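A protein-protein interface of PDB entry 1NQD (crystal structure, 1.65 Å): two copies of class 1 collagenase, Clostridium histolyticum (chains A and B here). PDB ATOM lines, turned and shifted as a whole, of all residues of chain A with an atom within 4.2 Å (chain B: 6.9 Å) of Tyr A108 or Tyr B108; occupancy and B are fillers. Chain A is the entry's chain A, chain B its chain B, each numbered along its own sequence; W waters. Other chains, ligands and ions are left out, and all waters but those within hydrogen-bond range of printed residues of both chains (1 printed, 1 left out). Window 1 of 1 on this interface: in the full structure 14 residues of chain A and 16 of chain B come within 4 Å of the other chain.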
ATOM      1  N   SER A  42      11.408   3.452  -0.984  1.00  0.00           N
ATOM      2  CA  SER A  42      10.251   4.300  -1.213  1.00  0.00           C
ATOM      3  C   SER A  42       9.197   4.162  -0.112  1.00  0.00           C
ATOM      4  O   SER A  42       8.207   4.882  -0.198  1.00  0.00           O
ATOM      5  CB  SER A  42       9.552   3.994  -2.537  1.00  0.00           C
ATOM      6  OG  SER A  42       9.111   2.658  -2.615  1.00  0.00           O
ATOM      7  N   ARG A  43       9.436   3.246   0.823  1.00  0.00           N
ATOM      8  CA  ARG A  43       8.467   3.025   1.885  1.00  0.00           C
ATOM      9  C   ARG A  43       9.167   2.792   3.212  1.00  0.00           C
ATOM     10  O   ARG A  43      10.106   2.005   3.297  1.00  0.00           O
ATOM     11  CB  ARG A  43       7.583   1.790   1.593  1.00  0.00           C
ATOM     12  CG  ARG A  43       6.993   1.803   0.190  1.00  0.00           C
ATOM     13  CD  ARG A  43       6.451   0.460  -0.232  1.00  0.00           C
ATOM     14  NE  ARG A  43       5.649  -0.271   0.726  1.00  0.00           N
ATOM     15  CZ  ARG A  43       4.328  -0.366   0.780  1.00  0.00           C
ATOM     16  NH1 ARG A  43       3.518   0.245  -0.085  1.00  0.00           N
ATOM     17  NH2 ARG A  43       3.791  -1.108   1.745  1.00  0.00           N
ATOM     18  N   VAL A  68       6.585  13.211  -0.829  1.00  0.00           N
ATOM     19  CA  VAL A  68       6.455  12.190   0.234  1.00  0.00           C
ATOM     20  C   VAL A  68       5.152  12.442   0.973  1.00  0.00           C
ATOM     21  O   VAL A  68       4.752  13.603   1.143  1.00  0.00           O
ATOM     22  CB  VAL A  68       7.668  12.178   1.170  1.00  0.00           C
ATOM     23  CG1 VAL A  68       7.916  13.527   1.825  1.00  0.00           C
ATOM     24  CG2 VAL A  68       7.510  11.106   2.253  1.00  0.00           C
ATOM     25  N   THR A  69       4.462  11.366   1.368  1.00  0.00           N
ATOM     26  CA  THR A  69       3.272  11.579   2.219  1.00  0.00           C
ATOM     27  C   THR A  69       3.173  10.359   3.126  1.00  0.00           C
ATOM     28  O   THR A  69       4.178   9.654   3.297  1.00  0.00           O
ATOM     29  CB  THR A  69       2.016  11.886   1.411  1.00  0.00           C
ATOM     30  OG1 THR A  69       0.844  12.093   2.244  1.00  0.00           O
ATOM     31  CG2 THR A  69       1.680  10.721   0.473  1.00  0.00           C
ATOM     32  N   TRP A  70       2.033  10.141   3.737  1.00  0.00           N
ATOM     33  CA  TRP A  70       1.910   9.021   4.675  1.00  0.00           C
ATOM     34  C   TRP A  70       0.455   8.588   4.756  1.00  0.00           C
ATOM     35  O   TRP A  70      -0.496   9.315   4.437  1.00  0.00           O
ATOM     36  CB  TRP A  70       2.471   9.350   6.055  1.00  0.00           C
ATOM     37  CG  TRP A  70       1.897  10.516   6.802  1.00  0.00           C
ATOM     38  CD1 TRP A  70       2.513  11.726   6.937  1.00  0.00           C
ATOM     39  CD2 TRP A  70       0.657  10.611   7.512  1.00  0.00           C
ATOM     40  NE1 TRP A  70       1.739  12.586   7.686  1.00  0.00           N
ATOM     41  CE2 TRP A  70       0.596  11.923   8.046  1.00  0.00           C
ATOM     42  CE3 TRP A  70      -0.405   9.726   7.747  1.00  0.00           C
ATOM     43  CZ2 TRP A  70      -0.496  12.349   8.800  1.00  0.00           C
ATOM     44  CZ3 TRP A  70      -1.489  10.168   8.497  1.00  0.00           C
ATOM     45  CH2 TRP A  70      -1.531  11.476   9.017  1.00  0.00           C
ATOM     46  N   THR A  71       0.299   7.335   5.208  1.00  0.00           N
ATOM     47  CA  THR A  71      -1.022   6.735   5.351  1.00  0.00           C
ATOM     48  C   THR A  71      -1.064   5.997   6.689  1.00  0.00           C
ATOM     49  O   THR A  71      -0.190   5.185   6.984  1.00  0.00           O
ATOM     50  CB  THR A  71      -1.308   5.746   4.214  1.00  0.00           C
ATOM     51  OG1 THR A  71      -1.377   6.500   2.978  1.00  0.00           O
ATOM     52  CG2 THR A  71      -2.633   5.038   4.416  1.00  0.00           C
ATOM     53  N   TYR A  84      -5.055   9.888   5.584  1.00  0.00           N
ATOM     54  CA  TYR A  84      -3.905  10.307   4.802  1.00  0.00           C
ATOM     55  C   TYR A  84      -3.306  11.614   5.302  1.00  0.00           C
ATOM     56  O   TYR A  84      -4.070  12.488   5.751  1.00  0.00           O
ATOM     57  CB  TYR A  84      -4.385  10.512   3.367  1.00  0.00           C
ATOM     58  CG  TYR A  84      -5.098   9.386   2.667  1.00  0.00           C
ATOM     59  CD1 TYR A  84      -6.342   9.520   2.088  1.00  0.00           C
ATOM     60  CD2 TYR A  84      -4.448   8.152   2.589  1.00  0.00           C
ATOM     61  CE1 TYR A  84      -7.009   8.487   1.437  1.00  0.00           C
ATOM     62  CE2 TYR A  84      -5.098   7.114   1.933  1.00  0.00           C
ATOM     63  CZ  TYR A  84      -6.338   7.264   1.371  1.00  0.00           C
ATOM     64  OH  TYR A  84      -6.942   6.205   0.719  1.00  0.00           O
ATOM     65  N   LEU A 106       2.492   4.293   7.400  1.00  0.00           N
ATOM     66  CA  LEU A 106       3.306   4.085   6.215  1.00  0.00           C
ATOM     67  C   LEU A 106       3.756   5.440   5.683  1.00  0.00           C
ATOM     68  O   LEU A 106       2.879   6.200   5.237  1.00  0.00           O
ATOM     69  CB  LEU A 106       2.453   3.325   5.200  1.00  0.00           C
ATOM     70  CG  LEU A 106       3.104   3.165   3.813  1.00  0.00           C
ATOM     71  CD1 LEU A 106       4.461   2.510   3.998  1.00  0.00           C
ATOM     72  CD2 LEU A 106       2.186   2.391   2.882  1.00  0.00           C
ATOM     73  N   VAL A 107       5.045   5.705   5.756  1.00  0.00           N
ATOM     74  CA  VAL A 107       5.607   6.895   5.104  1.00  0.00           C
ATOM     75  C   VAL A 107       6.094   6.435   3.728  1.00  0.00           C
ATOM     76  O   VAL A 107       6.833   5.463   3.645  1.00  0.00           O
ATOM     77  CB  VAL A 107       6.758   7.495   5.895  1.00  0.00           C
ATOM     78  CG1 VAL A 107       7.421   8.673   5.191  1.00  0.00           C
ATOM     79  CG2 VAL A 107       6.290   7.969   7.269  1.00  0.00           C
ATOM     80  N   TYR A 108       5.656   7.074   2.654  1.00  0.00           N
ATOM     81  CA  TYR A 108       6.026   6.601   1.321  1.00  0.00           C
ATOM     82  C   TYR A 108       6.153   7.789   0.381  1.00  0.00           C
ATOM     83  O   TYR A 108       5.593   8.856   0.570  1.00  0.00           O
ATOM     84  CB  TYR A 108       4.991   5.622   0.752  1.00  0.00           C
ATOM     85  CG  TYR A 108       3.670   6.241   0.423  1.00  0.00           C
ATOM     86  CD1 TYR A 108       3.367   6.636  -0.880  1.00  0.00           C
ATOM     87  CD2 TYR A 108       2.701   6.463   1.406  1.00  0.00           C
ATOM     88  CE1 TYR A 108       2.180   7.211  -1.250  1.00  0.00           C
ATOM     89  CE2 TYR A 108       1.490   7.046   1.043  1.00  0.00           C
ATOM     90  CZ  TYR A 108       1.230   7.416  -0.264  1.00  0.00           C
ATOM     91  OH  TYR A 108       0.021   8.000  -0.591  1.00  0.00           O
ATOM     92  N   LYS A 109       6.927   7.574  -0.683  1.00  0.00           N
ATOM     93  CA  LYS A 109       7.098   8.694  -1.615  1.00  0.00           C
ATOM     94  C   LYS A 109       6.470   8.365  -2.963  1.00  0.00           C
ATOM     95  O   LYS A 109       6.323   7.207  -3.336  1.00  0.00           O
ATOM     96  CB  LYS A 109       8.598   8.981  -1.747  1.00  0.00           C
ATOM     97  CG  LYS A 109       9.405   7.838  -2.357  1.00  0.00           C
ATOM     98  CD  LYS A 109      10.784   8.378  -2.770  1.00  0.00           C
ATOM     99  CE  LYS A 109      11.747   7.241  -3.091  1.00  0.00           C
ATOM    100  NZ  LYS A 109      13.119   7.762  -3.398  1.00  0.00           N
ATOM    101  N   LEU B  37      -0.537  -7.021  -6.587  1.00  0.00           N
ATOM    102  CA  LEU B  37       0.465  -6.593  -5.622  1.00  0.00           C
ATOM    103  C   LEU B  37       0.748  -7.733  -4.659  1.00  0.00           C
ATOM    104  O   LEU B  37       0.269  -7.739  -3.533  1.00  0.00           O
ATOM    105  CB  LEU B  37       0.021  -5.338  -4.854  1.00  0.00           C
ATOM    106  CG  LEU B  37       0.033  -4.079  -5.741  1.00  0.00           C
ATOM    107  CD1 LEU B  37      -0.926  -3.021  -5.162  1.00  0.00           C
ATOM    108  CD2 LEU B  37       1.430  -3.530  -5.858  1.00  0.00           C
ATOM    109  N   SER B  42       4.734  -4.058  -3.856  1.00  0.00           N
ATOM    110  CA  SER B  42       3.810  -3.208  -3.113  1.00  0.00           C
ATOM    111  C   SER B  42       3.485  -1.912  -3.837  1.00  0.00           C
ATOM    112  O   SER B  42       2.641  -1.163  -3.326  1.00  0.00           O
ATOM    113  CB  SER B  42       4.409  -2.868  -1.737  1.00  0.00           C
ATOM    114  OG  SER B  42       5.651  -2.191  -1.913  1.00  0.00           O
ATOM    115  N   ARG B  43       4.090  -1.640  -4.985  1.00  0.00           N
ATOM    116  CA  ARG B  43       3.673  -0.438  -5.707  1.00  0.00           C
ATOM    117  C   ARG B  43       3.596  -0.684  -7.213  1.00  0.00           C
ATOM    118  O   ARG B  43       4.515  -1.333  -7.695  1.00  0.00           O
ATOM    119  CB  ARG B  43       4.671   0.702  -5.495  1.00  0.00           C
ATOM    120  CG  ARG B  43       4.827   1.235  -4.090  1.00  0.00           C
ATOM    121  CD  ARG B  43       5.710   2.463  -4.017  1.00  0.00           C
ATOM    122  NE  ARG B  43       6.783   2.562  -5.000  1.00  0.00           N
ATOM    123  CZ  ARG B  43       7.294   3.736  -5.374  1.00  0.00           C
ATOM    124  NH1 ARG B  43       6.816   4.852  -4.840  1.00  0.00           N
ATOM    125  NH2 ARG B  43       8.271   3.830  -6.265  1.00  0.00           N
ATOM    126  N   ASP B  44       2.562  -0.178  -7.859  1.00  0.00           N
ATOM    127  CA  ASP B  44       2.420  -0.231  -9.310  1.00  0.00           C
ATOM    128  C   ASP B  44       2.169   1.194  -9.821  1.00  0.00           C
ATOM    129  O   ASP B  44       1.123   1.720  -9.473  1.00  0.00           O
ATOM    130  CB  ASP B  44       1.273  -1.141  -9.706  1.00  0.00           C
ATOM    131  CG  ASP B  44       1.572  -2.627  -9.502  1.00  0.00           C
ATOM    132  OD1 ASP B  44       2.722  -3.012  -9.256  1.00  0.00           O
ATOM    133  OD2 ASP B  44       0.559  -3.343  -9.463  1.00  0.00           O
ATOM    134  N   LEU B  60     -10.398   1.898  -8.585  1.00  0.00           N
ATOM    135  CA  LEU B  60      -9.631   0.673  -8.362  1.00  0.00           C
ATOM    136  C   LEU B  60     -10.629  -0.362  -7.833  1.00  0.00           C
ATOM    137  O   LEU B  60     -11.373  -0.082  -6.899  1.00  0.00           O
ATOM    138  CB  LEU B  60      -8.468   0.876  -7.396  1.00  0.00           C
ATOM    139  CG  LEU B  60      -7.648  -0.379  -7.100  1.00  0.00           C
ATOM    140  CD1 LEU B  60      -6.210  -0.039  -6.741  1.00  0.00           C
ATOM    141  CD2 LEU B  60      -8.320  -1.178  -5.982  1.00  0.00           C
ATOM    142  N   PHE B  66      -7.614  -7.047   0.394  1.00  0.00           N
ATOM    143  CA  PHE B  66      -6.311  -6.642   0.918  1.00  0.00           C
ATOM    144  C   PHE B  66      -6.341  -5.103   1.037  1.00  0.00           C
ATOM    145  O   PHE B  66      -7.305  -4.520   0.564  1.00  0.00           O
ATOM    146  CB  PHE B  66      -5.081  -7.078   0.172  1.00  0.00           C
ATOM    147  CG  PHE B  66      -4.796  -6.570  -1.230  1.00  0.00           C
ATOM    148  CD1 PHE B  66      -5.701  -6.768  -2.253  1.00  0.00           C
ATOM    149  CD2 PHE B  66      -3.592  -5.928  -1.468  1.00  0.00           C
ATOM    150  CE1 PHE B  66      -5.414  -6.302  -3.524  1.00  0.00           C
ATOM    151  CE2 PHE B  66      -3.287  -5.449  -2.738  1.00  0.00           C
ATOM    152  CZ  PHE B  66      -4.208  -5.674  -3.746  1.00  0.00           C
ATOM    153  N   GLY B  67      -5.336  -4.535   1.670  1.00  0.00           N
ATOM    154  CA  GLY B  67      -5.255  -3.100   1.880  1.00  0.00           C
ATOM    155  C   GLY B  67      -4.538  -2.399   0.747  1.00  0.00           C
ATOM    156  O   GLY B  67      -3.307  -2.411   0.671  1.00  0.00           O
ATOM    157  N   VAL B  68      -5.311  -1.790  -0.148  1.00  0.00           N
ATOM    158  CA  VAL B  68      -4.717  -1.173  -1.337  1.00  0.00           C
ATOM    159  C   VAL B  68      -5.425   0.161  -1.604  1.00  0.00           C
ATOM    160  O   VAL B  68      -6.629   0.256  -1.409  1.00  0.00           O
ATOM    161  CB  VAL B  68      -4.767  -2.142  -2.533  1.00  0.00           C
ATOM    162  CG1 VAL B  68      -6.188  -2.560  -2.900  1.00  0.00           C
ATOM    163  CG2 VAL B  68      -4.082  -1.553  -3.773  1.00  0.00           C
ATOM    164  N   THR B  69      -4.625   1.140  -2.017  1.00  0.00           N
ATOM    165  CA  THR B  69      -5.206   2.449  -2.377  1.00  0.00           C
ATOM    166  C   THR B  69      -4.345   3.098  -3.445  1.00  0.00           C
ATOM    167  O   THR B  69      -3.528   2.438  -4.117  1.00  0.00           O
ATOM    168  CB  THR B  69      -5.392   3.278  -1.106  1.00  0.00           C
ATOM    169  OG1 THR B  69      -6.106   4.477  -1.486  1.00  0.00           O
ATOM    170  CG2 THR B  69      -4.080   3.668  -0.453  1.00  0.00           C
ATOM    171  N   TRP B  70      -4.519   4.402  -3.682  1.00  0.00           N
ATOM    172  CA  TRP B  70      -3.731   5.021  -4.747  1.00  0.00           C
ATOM    173  C   TRP B  70      -3.598   6.526  -4.528  1.00  0.00           C
ATOM    174  O   TRP B  70      -4.378   7.147  -3.810  1.00  0.00           O
ATOM    175  CB  TRP B  70      -4.381   4.789  -6.114  1.00  0.00           C
ATOM    176  CG  TRP B  70      -5.810   5.158  -6.329  1.00  0.00           C
ATOM    177  CD1 TRP B  70      -6.898   4.320  -6.300  1.00  0.00           C
ATOM    178  CD2 TRP B  70      -6.334   6.473  -6.620  1.00  0.00           C
ATOM    179  NE1 TRP B  70      -8.053   5.037  -6.553  1.00  0.00           N
ATOM    180  CE2 TRP B  70      -7.724   6.350  -6.749  1.00  0.00           C
ATOM    181  CE3 TRP B  70      -5.738   7.733  -6.779  1.00  0.00           C
ATOM    182  CZ2 TRP B  70      -8.567   7.434  -7.034  1.00  0.00           C
ATOM    183  CZ3 TRP B  70      -6.561   8.816  -7.060  1.00  0.00           C
ATOM    184  CH2 TRP B  70      -7.957   8.666  -7.185  1.00  0.00           C
ATOM    185  N   THR B  71      -2.591   7.077  -5.172  1.00  0.00           N
ATOM    186  CA  THR B  71      -2.253   8.501  -5.086  1.00  0.00           C
ATOM    187  C   THR B  71      -1.942   9.038  -6.472  1.00  0.00           C
ATOM    188  O   THR B  71      -1.056   8.491  -7.133  1.00  0.00           O
ATOM    189  CB  THR B  71      -1.048   8.682  -4.158  1.00  0.00           C
ATOM    190  OG1 THR B  71      -1.501   8.240  -2.876  1.00  0.00           O
ATOM    191  CG2 THR B  71      -0.642  10.152  -4.029  1.00  0.00           C
ATOM    192  N   ILE B  82      -2.216  16.907  -4.749  1.00  0.00           N
ATOM    193  CA  ILE B  82      -2.277  15.452  -4.752  1.00  0.00           C
ATOM    194  C   ILE B  82      -3.702  14.952  -4.625  1.00  0.00           C
ATOM    195  O   ILE B  82      -4.488  15.602  -3.928  1.00  0.00           O
ATOM    196  CB  ILE B  82      -1.374  14.931  -3.614  1.00  0.00           C
ATOM    197  CG1 ILE B  82       0.024  15.563  -3.668  1.00  0.00           C
ATOM    198  CG2 ILE B  82      -1.298  13.421  -3.623  1.00  0.00           C
ATOM    199  CD1 ILE B  82       0.752  15.144  -4.934  1.00  0.00           C
ATOM    200  N   TYR B  84      -6.133  11.512  -3.484  1.00  0.00           N
ATOM    201  CA  TYR B  84      -6.056  10.159  -2.932  1.00  0.00           C
ATOM    202  C   TYR B  84      -7.308   9.365  -3.263  1.00  0.00           C
ATOM    203  O   TYR B  84      -8.414   9.889  -3.343  1.00  0.00           O
ATOM    204  CB  TYR B  84      -5.954  10.206  -1.401  1.00  0.00           C
ATOM    205  CG  TYR B  84      -4.774  10.931  -0.834  1.00  0.00           C
ATOM    206  CD1 TYR B  84      -4.980  11.984   0.067  1.00  0.00           C
ATOM    207  CD2 TYR B  84      -3.468  10.620  -1.183  1.00  0.00           C
ATOM    208  CE1 TYR B  84      -3.897  12.655   0.579  1.00  0.00           C
ATOM    209  CE2 TYR B  84      -2.369  11.283  -0.666  1.00  0.00           C
ATOM    210  CZ  TYR B  84      -2.607  12.324   0.238  1.00  0.00           C
ATOM    211  OH  TYR B  84      -1.523  12.994   0.758  1.00  0.00           O
ATOM    212  N   LEU B 106      -0.136   6.267  -8.624  1.00  0.00           N
ATOM    213  CA  LEU B 106       0.561   5.261  -7.837  1.00  0.00           C
ATOM    214  C   LEU B 106      -0.439   4.337  -7.162  1.00  0.00           C
ATOM    215  O   LEU B 106      -1.222   4.813  -6.338  1.00  0.00           O
ATOM    216  CB  LEU B 106       1.430   5.915  -6.760  1.00  0.00           C
ATOM    217  CG  LEU B 106       2.210   4.979  -5.825  1.00  0.00           C
ATOM    218  CD1 LEU B 106       2.986   3.939  -6.638  1.00  0.00           C
ATOM    219  CD2 LEU B 106       3.172   5.754  -4.938  1.00  0.00           C
ATOM    220  N   VAL B 107      -0.454   3.064  -7.516  1.00  0.00           N
ATOM    221  CA  VAL B 107      -1.335   2.127  -6.816  1.00  0.00           C
ATOM    222  C   VAL B 107      -0.451   1.447  -5.780  1.00  0.00           C
ATOM    223  O   VAL B 107       0.608   0.959  -6.161  1.00  0.00           O
ATOM    224  CB  VAL B 107      -1.947   1.072  -7.736  1.00  0.00           C
ATOM    225  CG1 VAL B 107      -2.712   0.027  -6.933  1.00  0.00           C
ATOM    226  CG2 VAL B 107      -2.861   1.739  -8.759  1.00  0.00           C
ATOM    227  N   TYR B 108      -0.806   1.416  -4.501  1.00  0.00           N
ATOM    228  CA  TYR B 108       0.195   0.886  -3.572  1.00  0.00           C
ATOM    229  C   TYR B 108      -0.570   0.155  -2.469  1.00  0.00           C
ATOM    230  O   TYR B 108      -1.731   0.458  -2.198  1.00  0.00           O
ATOM    231  CB  TYR B 108       1.129   1.934  -2.969  1.00  0.00           C
ATOM    232  CG  TYR B 108       0.414   2.902  -2.046  1.00  0.00           C
ATOM    233  CD1 TYR B 108       0.361   2.695  -0.665  1.00  0.00           C
ATOM    234  CD2 TYR B 108      -0.227   4.031  -2.549  1.00  0.00           C
ATOM    235  CE1 TYR B 108      -0.302   3.594   0.158  1.00  0.00           C
ATOM    236  CE2 TYR B 108      -0.895   4.928  -1.736  1.00  0.00           C
ATOM    237  CZ  TYR B 108      -0.930   4.706  -0.361  1.00  0.00           C
ATOM    238  OH  TYR B 108      -1.603   5.603   0.425  1.00  0.00           O
ATOM    239  N   LYS B 109       0.077  -0.817  -1.829  1.00  0.00           N
ATOM    240  CA  LYS B 109      -0.664  -1.489  -0.760  1.00  0.00           C
ATOM    241  C   LYS B 109      -0.127  -1.116   0.630  1.00  0.00           C
ATOM    242  O   LYS B 109       0.989  -0.613   0.764  1.00  0.00           O
ATOM    243  CB  LYS B 109      -0.667  -3.010  -0.930  1.00  0.00           C
ATOM    244  CG  LYS B 109       0.711  -3.642  -1.003  1.00  0.00           C
ATOM    245  CD  LYS B 109       0.522  -5.175  -0.987  1.00  0.00           C
ATOM    246  CE  LYS B 109       1.865  -5.873  -0.989  1.00  0.00           C
ATOM    247  NZ  LYS B 109       1.672  -7.368  -1.032  1.00  0.00           N
ATOM    248  N   TYR B 110      -0.972  -1.374   1.630  1.00  0.00           N
ATOM    249  CA  TYR B 110      -0.561  -1.124   3.021  1.00  0.00           C
ATOM    250  C   TYR B 110      -0.814  -2.350   3.876  1.00  0.00           C
ATOM    251  O   TYR B 110      -0.503  -2.410   5.069  1.00  0.00           O
ATOM    252  CB  TYR B 110      -1.277   0.101   3.592  1.00  0.00           C
ATOM    253  CG  TYR B 110      -2.768   0.088   3.459  1.00  0.00           C
ATOM    254  CD1 TYR B 110      -3.589  -0.531   4.394  1.00  0.00           C
ATOM    255  CD2 TYR B 110      -3.407   0.716   2.384  1.00  0.00           C
ATOM    256  CE1 TYR B 110      -4.952  -0.530   4.263  1.00  0.00           C
ATOM    257  CE2 TYR B 110      -4.775   0.713   2.245  1.00  0.00           C
ATOM    258  CZ  TYR B 110      -5.563   0.090   3.195  1.00  0.00           C
ATOM    259  OH  TYR B 110      -6.920   0.079   3.066  1.00  0.00           O
ATOM    260  N   SER B 111      -1.382  -3.383   3.260  1.00  0.00           N
ATOM    261  CA  SER B 111      -1.615  -4.624   4.008  1.00  0.00           C
ATOM    262  C   SER B 111      -1.988  -5.753   3.057  1.00  0.00           C
ATOM    263  O   SER B 111      -2.650  -5.536   2.045  1.00  0.00           O
ATOM    264  CB  SER B 111      -2.695  -4.446   5.070  1.00  0.00           C
ATOM    265  OG  SER B 111      -4.003  -4.506   4.531  1.00  0.00           O
ATOM    266  N   TYR B 116      -6.093  -6.575  -8.495  1.00  0.00           N
ATOM    267  CA  TYR B 116      -7.017  -5.467  -8.640  1.00  0.00           C
ATOM    268  C   TYR B 116      -7.162  -5.175 -10.132  1.00  0.00           C
ATOM    269  O   TYR B 116      -6.339  -5.667 -10.920  1.00  0.00           O
ATOM    270  CB  TYR B 116      -6.542  -4.198  -7.908  1.00  0.00           C
ATOM    271  CG  TYR B 116      -5.230  -3.713  -8.495  1.00  0.00           C
ATOM    272  CD1 TYR B 116      -5.217  -2.732  -9.497  1.00  0.00           C
ATOM    273  CD2 TYR B 116      -4.035  -4.251  -8.057  1.00  0.00           C
ATOM    274  CE1 TYR B 116      -3.993  -2.323  -9.999  1.00  0.00           C
ATOM    275  CE2 TYR B 116      -2.798  -3.855  -8.572  1.00  0.00           C
ATOM    276  CZ  TYR B 116      -2.812  -2.885  -9.551  1.00  0.00           C
ATOM    277  OH  TYR B 116      -1.600  -2.477 -10.072  1.00  0.00           O
HETATM  278  O   HOH W   1      -3.280   7.277  -0.798  1.00  0.00           O
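Tyr A108 touches just these residues of chain B: Thr B71 and Tyr B108. Tyr B108 touches just these residues of chain A: Thr A71 (2.7 Å), Leu A106 (3.9 Å) and Tyr A108 (3.1 Å). Of the printed residues of chain B, Leu A106 touches Tyr B108 and Lys B109. Of the printed residues of chain A, Lys B109 touches Arg A43 and Leu A106. Printed residues of chain A within 4 Å of Thr B69: Tyr A84. Of the printed residues of chain A, Tyr B84 touches Thr A69 (2.9 Å) and Tyr A84 (3.5 Å). The nearest printed residue of chain B that does not touch Tyr A108 is Tyr B84 (4.1 Å). The nearest residue of chain A that does not touch Tyr B108 is Arg A43 (4.04 Å). The nearest printed residue of chain B that does not touch Leu A106 is Tyr B110 (4.2 Å).
Printed residues of chain A that touch a printed residue of chain B: Ser A42, Arg A43, Thr A69, Thr A71, Tyr A84, Leu A106, Tyr A108 and Lys A109. Of the 20 printed residues of chain B, 8 touch a printed residue of chain A. Among the printed residues, 13 pairs touch across the chains.
Among the printed residues, merely in contact across the chains: Tyr A84 with Tyr B84 (3.5 Å), Leu A106 with Tyr B108 (3.9 Å), Leu A106 with Lys B109 (3.9 Å) and Lys A109 with Leu B106 (3.8 Å).
Thr A71 touches Tyr B108, and with the chains exchanged Tyr A108 touches Thr B71. Tyr A84 touches its own counterpart, Tyr B84. Leu A106 touches Tyr B108, but with the chains exchanged Tyr A108 does not touch Leu B106 (4.1 Å). Leu A106 touches Lys B109, and with the chains exchanged Lys A109 touches Leu B106. 11 positions are printed for both chains. Of the 13 pairs that touch across the chains among the printed residues, 12 have their exchanged pair printed and touching as well.
N of Thr A69 sits at hydrogen-bond distance from O of Tyr A108, 2.9 Å away. N of Thr A71 is in hydrogen-bond range of O of Leu A106. O of Leu B37 lies within hydrogen-bond range of NZ of Lys B109 (2.9 Å). The backbone NH of Lys B109 is in hydrogen-bond range of the backbone carbonyl oxygen of Ser B42, at 3.0 Å. O of Thr B69 lies within hydrogen-bond range of N of Tyr B108, at 2.9 Å. The backbone carbonyl oxygen (O) of Thr B71 sits at hydrogen-bond distance from the backbone NH (N) of Leu B106 (2.8 Å).
Water W1 lies within hydrogen-bond range of the side-chain hydroxyl of Tyr B108 (2.7 Å), the side-chain hydroxyl of Thr B71 (2.9 Å), the backbone carbonyl oxygen of Trp B70 (3.2 Å) and the side-chain hydroxyl of Tyr A108 (3.4 Å).
The side-chain hydroxyl of Ser A42 sits at hydrogen-bond distance from the guanidinium group of Arg B43 (3.3 Å). NE of Arg A43 sits close to OG of Ser B42, 3.3 Å away. The backbone carbonyl oxygen (O) of Lys B109 sits at hydrogen-bond distance from the guanidinium group (NH1) of Arg A43, 2.8 Å away. OG1 of Thr A69 lies within hydrogen-bond range of OH of Tyr B84, at 2.9 Å. The side-chain hydroxyl (OH) of Tyr B108 lies within hydrogen-bond range of the side-chain hydroxyl (OG1) of Thr A71 (2.7 Å). The side-chain hydroxyl of Tyr A84 is in hydrogen-bond range of the side-chain hydroxyl of Thr B69. The side-chain hydroxyl (OH) of Tyr A108 sits at hydrogen-bond distance from the side-chain hydroxyl (OG1) of Thr B71 (2.8 Å). OH of Tyr B108 lies within hydrogen-bond range of OH of Tyr A108. The backbone carbonyl oxygen (O) of Lys A109 sits at hydrogen-bond distance from the guanidinium group (NH1) of Arg B43 (2.8 Å).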
